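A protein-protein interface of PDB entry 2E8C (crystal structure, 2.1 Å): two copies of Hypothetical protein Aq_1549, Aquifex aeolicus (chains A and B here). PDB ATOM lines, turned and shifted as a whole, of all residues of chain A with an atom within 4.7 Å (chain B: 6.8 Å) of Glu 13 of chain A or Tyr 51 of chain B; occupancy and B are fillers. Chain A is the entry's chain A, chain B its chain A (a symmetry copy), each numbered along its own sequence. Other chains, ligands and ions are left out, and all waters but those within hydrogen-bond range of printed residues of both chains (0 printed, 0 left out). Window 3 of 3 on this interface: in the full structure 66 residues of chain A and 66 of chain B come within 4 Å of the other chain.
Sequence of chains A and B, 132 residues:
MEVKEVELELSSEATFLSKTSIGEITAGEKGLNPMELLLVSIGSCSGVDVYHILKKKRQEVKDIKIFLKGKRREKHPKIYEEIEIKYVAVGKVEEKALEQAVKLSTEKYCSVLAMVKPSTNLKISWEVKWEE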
ATOM      1  N   LEU A  10       8.596 -17.549  -6.006  1.00  0.00           N
ATOM      2  CA  LEU A  10       8.625 -18.442  -7.154  1.00  0.00           C
ATOM      3  C   LEU A  10       9.916 -18.227  -7.947  1.00  0.00           C
ATOM      4  O   LEU A  10      10.277 -17.089  -8.246  1.00  0.00           O
ATOM      5  CB  LEU A  10       7.400 -18.175  -8.033  1.00  0.00           C
ATOM      6  CG  LEU A  10       6.995 -19.251  -9.039  1.00  0.00           C
ATOM      7  CD1 LEU A  10       6.675 -20.554  -8.301  1.00  0.00           C
ATOM      8  CD2 LEU A  10       5.783 -18.770  -9.839  1.00  0.00           C
ATOM      9  N   SER A  12      11.012 -21.065 -10.383  1.00  0.00           N
ATOM     10  CA  SER A  12      10.751 -21.847 -11.585  1.00  0.00           C
ATOM     11  C   SER A  12       9.387 -22.489 -11.332  1.00  0.00           C
ATOM     12  O   SER A  12       8.777 -22.236 -10.290  1.00  0.00           O
ATOM     13  CB  SER A  12      11.827 -22.921 -11.790  1.00  0.00           C
ATOM     14  OG  SER A  12      11.811 -23.873 -10.742  1.00  0.00           O
ATOM     15  N   GLU A  13       8.907 -23.309 -12.265  1.00  0.00           N
ATOM     16  CA  GLU A  13       7.596 -23.943 -12.109  1.00  0.00           C
ATOM     17  C   GLU A  13       7.431 -24.670 -10.778  1.00  0.00           C
ATOM     18  O   GLU A  13       8.175 -25.600 -10.478  1.00  0.00           O
ATOM     19  CB  GLU A  13       7.329 -24.944 -13.239  1.00  0.00           C
ATOM     20  CG  GLU A  13       5.853 -25.322 -13.358  1.00  0.00           C
ATOM     21  CD  GLU A  13       5.627 -26.711 -13.927  1.00  0.00           C
ATOM     22  OE1 GLU A  13       5.991 -27.692 -13.247  1.00  0.00           O
ATOM     23  OE2 GLU A  13       5.083 -26.824 -15.049  1.00  0.00           O
ATOM     24  N   ALA A  14       6.438 -24.249  -9.997  1.00  0.00           N
ATOM     25  CA  ALA A  14       6.145 -24.855  -8.697  1.00  0.00           C
ATOM     26  C   ALA A  14       7.389 -25.023  -7.825  1.00  0.00           C
ATOM     27  O   ALA A  14       7.497 -25.982  -7.063  1.00  0.00           O
ATOM     28  CB  ALA A  14       5.459 -26.210  -8.897  1.00  0.00           C
ATOM     29  N   THR A  15       8.322 -24.086  -7.942  1.00  0.00           N
ATOM     30  CA  THR A  15       9.553 -24.118  -7.161  1.00  0.00           C
ATOM     31  C   THR A  15       9.741 -22.742  -6.541  1.00  0.00           C
ATOM     32  O   THR A  15       9.290 -21.740  -7.098  1.00  0.00           O
ATOM     33  CB  THR A  15      10.760 -24.475  -8.048  1.00  0.00           C
ATOM     34  OG1 THR A  15      10.474 -25.685  -8.761  1.00  0.00           O
ATOM     35  CG2 THR A  15      12.008 -24.693  -7.196  1.00  0.00           C
ATOM     36  N   GLU A  29       8.987 -28.505  -6.700  1.00  0.00           N
ATOM     37  CA  GLU A  29       8.956 -29.494  -7.765  1.00  0.00           C
ATOM     38  C   GLU A  29      10.274 -29.682  -8.517  1.00  0.00           C
ATOM     39  O   GLU A  29      10.618 -30.801  -8.893  1.00  0.00           O
ATOM     40  CB  GLU A  29       7.848 -29.126  -8.747  1.00  0.00           C
ATOM     41  CG  GLU A  29       7.561 -30.169  -9.793  1.00  0.00           C
ATOM     42  CD  GLU A  29       6.398 -29.771 -10.670  1.00  0.00           C
ATOM     43  OE1 GLU A  29       5.285 -29.600 -10.131  1.00  0.00           O
ATOM     44  OE2 GLU A  29       6.598 -29.625 -11.894  1.00  0.00           O
ATOM     45  N   LYS A  30      11.004 -28.596  -8.746  1.00  0.00           N
ATOM     46  CA  LYS A  30      12.272 -28.680  -9.464  1.00  0.00           C
ATOM     47  C   LYS A  30      13.475 -28.388  -8.575  1.00  0.00           C
ATOM     48  O   LYS A  30      14.565 -28.109  -9.069  1.00  0.00           O
ATOM     49  CB  LYS A  30      12.275 -27.707 -10.647  1.00  0.00           C
ATOM     50  CG  LYS A  30      11.246 -28.024 -11.714  1.00  0.00           C
ATOM     51  CD  LYS A  30      11.337 -27.026 -12.854  1.00  0.00           C
ATOM     52  CE  LYS A  30      10.344 -27.348 -13.957  1.00  0.00           C
ATOM     53  NZ  LYS A  30      10.479 -26.398 -15.104  1.00  0.00           N
ATOM     54  N   SER B  46       3.278 -26.224   0.625  1.00  0.00           N
ATOM     55  CA  SER B  46       2.036 -25.514   0.368  1.00  0.00           C
ATOM     56  C   SER B  46       2.176 -24.724  -0.929  1.00  0.00           C
ATOM     57  O   SER B  46       1.261 -24.697  -1.748  1.00  0.00           O
ATOM     58  CB  SER B  46       1.715 -24.578   1.533  1.00  0.00           C
ATOM     59  OG  SER B  46       0.439 -23.977   1.363  1.00  0.00           O
ATOM     60  N   GLY B  47       3.335 -24.096  -1.111  1.00  0.00           N
ATOM     61  CA  GLY B  47       3.582 -23.320  -2.312  1.00  0.00           C
ATOM     62  C   GLY B  47       3.362 -24.135  -3.573  1.00  0.00           C
ATOM     63  O   GLY B  47       2.819 -23.633  -4.558  1.00  0.00           O
ATOM     64  N   VAL B  48       3.792 -25.393  -3.555  1.00  0.00           N
ATOM     65  CA  VAL B  48       3.613 -26.273  -4.706  1.00  0.00           C
ATOM     66  C   VAL B  48       2.112 -26.462  -4.966  1.00  0.00           C
ATOM     67  O   VAL B  48       1.670 -26.426  -6.117  1.00  0.00           O
ATOM     68  CB  VAL B  48       4.280 -27.648  -4.462  1.00  0.00           C
ATOM     69  CG1 VAL B  48       3.896 -28.629  -5.564  1.00  0.00           C
ATOM     70  CG2 VAL B  48       5.797 -27.484  -4.414  1.00  0.00           C
ATOM     71  N   ASP B  49       1.333 -26.653  -3.899  1.00  0.00           N
ATOM     72  CA  ASP B  49      -0.117 -26.818  -4.032  1.00  0.00           C
ATOM     73  C   ASP B  49      -0.754 -25.573  -4.650  1.00  0.00           C
ATOM     74  O   ASP B  49      -1.489 -25.653  -5.636  1.00  0.00           O
ATOM     75  CB  ASP B  49      -0.787 -27.045  -2.670  1.00  0.00           C
ATOM     76  CG  ASP B  49      -0.347 -28.320  -1.991  1.00  0.00           C
ATOM     77  OD1 ASP B  49      -0.031 -29.313  -2.680  1.00  0.00           O
ATOM     78  OD2 ASP B  49      -0.348 -28.332  -0.743  1.00  0.00           O
ATOM     79  N   VAL B  50      -0.483 -24.419  -4.050  1.00  0.00           N
ATOM     80  CA  VAL B  50      -1.050 -23.163  -4.527  1.00  0.00           C
ATOM     81  C   VAL B  50      -0.724 -22.907  -5.994  1.00  0.00           C
ATOM     82  O   VAL B  50      -1.586 -22.487  -6.763  1.00  0.00           O
ATOM     83  CB  VAL B  50      -0.559 -21.975  -3.673  1.00  0.00           C
ATOM     84  CG1 VAL B  50      -1.013 -20.658  -4.290  1.00  0.00           C
ATOM     85  CG2 VAL B  50      -1.111 -22.102  -2.258  1.00  0.00           C
ATOM     86  N   TYR B  51       0.517 -23.165  -6.388  1.00  0.00           N
ATOM     87  CA  TYR B  51       0.917 -22.954  -7.772  1.00  0.00           C
ATOM     88  C   TYR B  51       0.066 -23.794  -8.725  1.00  0.00           C
ATOM     89  O   TYR B  51      -0.541 -23.269  -9.660  1.00  0.00           O
ATOM     90  CB  TYR B  51       2.382 -23.320  -7.966  1.00  0.00           C
ATOM     91  CG  TYR B  51       2.850 -23.150  -9.386  1.00  0.00           C
ATOM     92  CD1 TYR B  51       3.329 -21.924  -9.839  1.00  0.00           C
ATOM     93  CD2 TYR B  51       2.806 -24.217 -10.286  1.00  0.00           C
ATOM     94  CE1 TYR B  51       3.758 -21.763 -11.154  1.00  0.00           C
ATOM     95  CE2 TYR B  51       3.231 -24.067 -11.602  1.00  0.00           C
ATOM     96  CZ  TYR B  51       3.706 -22.839 -12.028  1.00  0.00           C
ATOM     97  OH  TYR B  51       4.140 -22.690 -13.326  1.00  0.00           O
ATOM     98  N   HIS B  52       0.025 -25.100  -8.488  1.00  0.00           N
ATOM     99  CA  HIS B  52      -0.747 -25.999  -9.339  1.00  0.00           C
ATOM    100  C   HIS B  52      -2.240 -25.697  -9.347  1.00  0.00           C
ATOM    101  O   HIS B  52      -2.884 -25.754 -10.396  1.00  0.00           O
ATOM    102  CB  HIS B  52      -0.523 -27.451  -8.918  1.00  0.00           C
ATOM    103  CG  HIS B  52       0.853 -27.954  -9.221  1.00  0.00           C
ATOM    104  ND1 HIS B  52       1.391 -27.923 -10.489  1.00  0.00           N
ATOM    105  CD2 HIS B  52       1.808 -28.485  -8.419  1.00  0.00           C
ATOM    106  CE1 HIS B  52       2.619 -28.409 -10.456  1.00  0.00           C
ATOM    107  NE2 HIS B  52       2.896 -28.757  -9.213  1.00  0.00           N
ATOM    108  N   ILE B  53      -2.790 -25.375  -8.182  1.00  0.00           N
ATOM    109  CA  ILE B  53      -4.212 -25.073  -8.088  1.00  0.00           C
ATOM    110  C   ILE B  53      -4.550 -23.785  -8.835  1.00  0.00           C
ATOM    111  O   ILE B  53      -5.503 -23.749  -9.612  1.00  0.00           O
ATOM    112  CB  ILE B  53      -4.666 -24.965  -6.613  1.00  0.00           C
ATOM    113  CG1 ILE B  53      -4.559 -26.341  -5.944  1.00  0.00           C
ATOM    114  CG2 ILE B  53      -6.104 -24.454  -6.544  1.00  0.00           C
ATOM    115  CD1 ILE B  53      -4.804 -26.337  -4.444  1.00  0.00           C
ATOM    116  N   LEU B  54      -3.772 -22.732  -8.610  1.00  0.00           N
ATOM    117  CA  LEU B  54      -4.015 -21.468  -9.299  1.00  0.00           C
ATOM    118  C   LEU B  54      -3.929 -21.665 -10.811  1.00  0.00           C
ATOM    119  O   LEU B  54      -4.684 -21.054 -11.570  1.00  0.00           O
ATOM    120  CB  LEU B  54      -3.001 -20.407  -8.862  1.00  0.00           C
ATOM    121  CG  LEU B  54      -3.149 -19.824  -7.455  1.00  0.00           C
ATOM    122  CD1 LEU B  54      -2.041 -18.810  -7.208  1.00  0.00           C
ATOM    123  CD2 LEU B  54      -4.514 -19.163  -7.311  1.00  0.00           C
ATOM    124  N   LYS B  55      -3.010 -22.523 -11.245  1.00  0.00           N
ATOM    125  CA  LYS B  55      -2.846 -22.790 -12.667  1.00  0.00           C
ATOM    126  C   LYS B  55      -4.054 -23.548 -13.212  1.00  0.00           C
ATOM    127  O   LYS B  55      -4.550 -23.247 -14.296  1.00  0.00           O
ATOM    128  CB  LYS B  55      -1.568 -23.597 -12.913  1.00  0.00           C
ATOM    129  CG  LYS B  55      -1.354 -23.998 -14.360  1.00  0.00           C
ATOM    130  CD  LYS B  55       0.018 -24.625 -14.550  1.00  0.00           C
ATOM    131  CE  LYS B  55       0.193 -25.174 -15.957  1.00  0.00           C
ATOM    132  NZ  LYS B  55      -0.721 -26.323 -16.225  1.00  0.00           N
ATOM    133  N   LYS B  56      -4.525 -24.529 -12.451  1.00  0.00           N
ATOM    134  CA  LYS B  56      -5.674 -25.319 -12.860  1.00  0.00           C
ATOM    135  C   LYS B  56      -6.906 -24.430 -12.971  1.00  0.00           C
ATOM    136  O   LYS B  56      -7.757 -24.636 -13.838  1.00  0.00           O
ATOM    137  CB  LYS B  56      -5.939 -26.439 -11.851  1.00  0.00           C
ATOM    138  CG  LYS B  56      -7.200 -27.238 -12.139  1.00  0.00           C
ATOM    139  CD  LYS B  56      -7.378 -28.387 -11.157  1.00  0.00           C
ATOM    140  CE  LYS B  56      -8.719 -29.079 -11.358  1.00  0.00           C
ATOM    141  NZ  LYS B  56      -9.857 -28.138 -11.139  1.00  0.00           N
ATOM    142  N   VAL B  61      -0.306 -16.471 -13.186  1.00  0.00           N
ATOM    143  CA  VAL B  61       0.641 -16.189 -12.118  1.00  0.00           C
ATOM    144  C   VAL B  61       1.970 -15.628 -12.597  1.00  0.00           C
ATOM    145  O   VAL B  61       2.681 -16.261 -13.374  1.00  0.00           O
ATOM    146  CB  VAL B  61       0.926 -17.460 -11.296  1.00  0.00           C
ATOM    147  CG1 VAL B  61       1.893 -17.143 -10.161  1.00  0.00           C
ATOM    148  CG2 VAL B  61      -0.382 -18.029 -10.759  1.00  0.00           C
ATOM    149  N   ILE B  64       4.682 -15.773  -6.872  1.00  0.00           N
ATOM    150  CA  ILE B  64       4.016 -16.178  -5.639  1.00  0.00           C
ATOM    151  C   ILE B  64       5.011 -16.004  -4.503  1.00  0.00           C
ATOM    152  O   ILE B  64       6.086 -16.608  -4.507  1.00  0.00           O
ATOM    153  CB  ILE B  64       3.561 -17.661  -5.676  1.00  0.00           C
ATOM    154  CG1 ILE B  64       2.545 -17.881  -6.803  1.00  0.00           C
ATOM    155  CG2 ILE B  64       2.932 -18.039  -4.338  1.00  0.00           C
ATOM    156  CD1 ILE B  64       2.172 -19.340  -7.016  1.00  0.00           C
ATOM    157  N   ALA B 101      -7.126 -21.979  -3.362  1.00  0.00           N
ATOM    158  CA  ALA B 101      -5.831 -22.649  -3.429  1.00  0.00           C
ATOM    159  C   ALA B 101      -5.211 -22.784  -2.046  1.00  0.00           C
ATOM    160  O   ALA B 101      -4.692 -23.841  -1.691  1.00  0.00           O
ATOM    161  CB  ALA B 101      -4.894 -21.883  -4.345  1.00  0.00           C
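The side-chain carboxylate (OE1) of Glu 29 of chain A lies within hydrogen-bond range of a ring nitrogen (NE2) of His 52 of chain B (2.7 Å). O of Ile 64 of chain B is in hydrogen-bond range of N of Leu 10 of chain A.
N of Glu 29 of chain A is in hydrogen-bond range of O of Ala 14 of chain A (3.0 Å). OE1 of Glu 13 of chain A sits close to OE2 of Glu 29 of chain A. OG1 of Thr 15 of chain A is in hydrogen-bond range of O of Glu 13 of chain A (2.9 Å).
Among the printed residues, pairs that only touch across the chains: Glu 13 of chain A with Tyr 51 of chain B (3.1 Å), Ala 14 of chain A with Val 48 of chain B (3.5 Å), Ala 14 of chain A with Tyr 51 of chain B (3.6 Å), Ala 14 of chain A with His 52 of chain B (3.6 Å) and Leu 10 of chain A with Tyr 51 of chain B (3.8 Å).
Of the printed residues of chain B, Leu 10 of chain A touches Tyr 51 and Ile 64. Glu 13 of chain A touches one residue of chain B. Printed residues of chain B within 4 Å of Ala 14 of chain A: Val 48, Tyr 51 and His 52. Of the printed residues of chain A, Val 48 of chain B touches Ala 14 (3.5 Å). Tyr 51 of chain B touches three residues of chain A. Of the printed residues of chain A, His 52 of chain B touches Ala 14 and Glu 29. Of the printed residues of chain A, Ile 64 of chain B touches Leu 10. The nearest residue of chain B that does not touch Glu 13 of chain A is His 52 of chain B (4.4 Å).
Hydrophobic or aromatic side chains of chain A within 4 Å of the printed part of chain B: Leu 10 and Ala 14. Along chain A the printed residues that touch a printed residue of chain B span positions 10 to 29. Of the 14 printed residues of chain B, 4 touch a printed residue of chain A. Hydrophobic or aromatic side chains of chain B within 4 Å of the printed part of chain A: Val 48, Tyr 51 and His 52. Among the printed residues, no Asp or Glu carboxylate lies within 4 Å of a Lys or Arg side-chain nitrogen of the other chain.
No position is printed for both chains.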
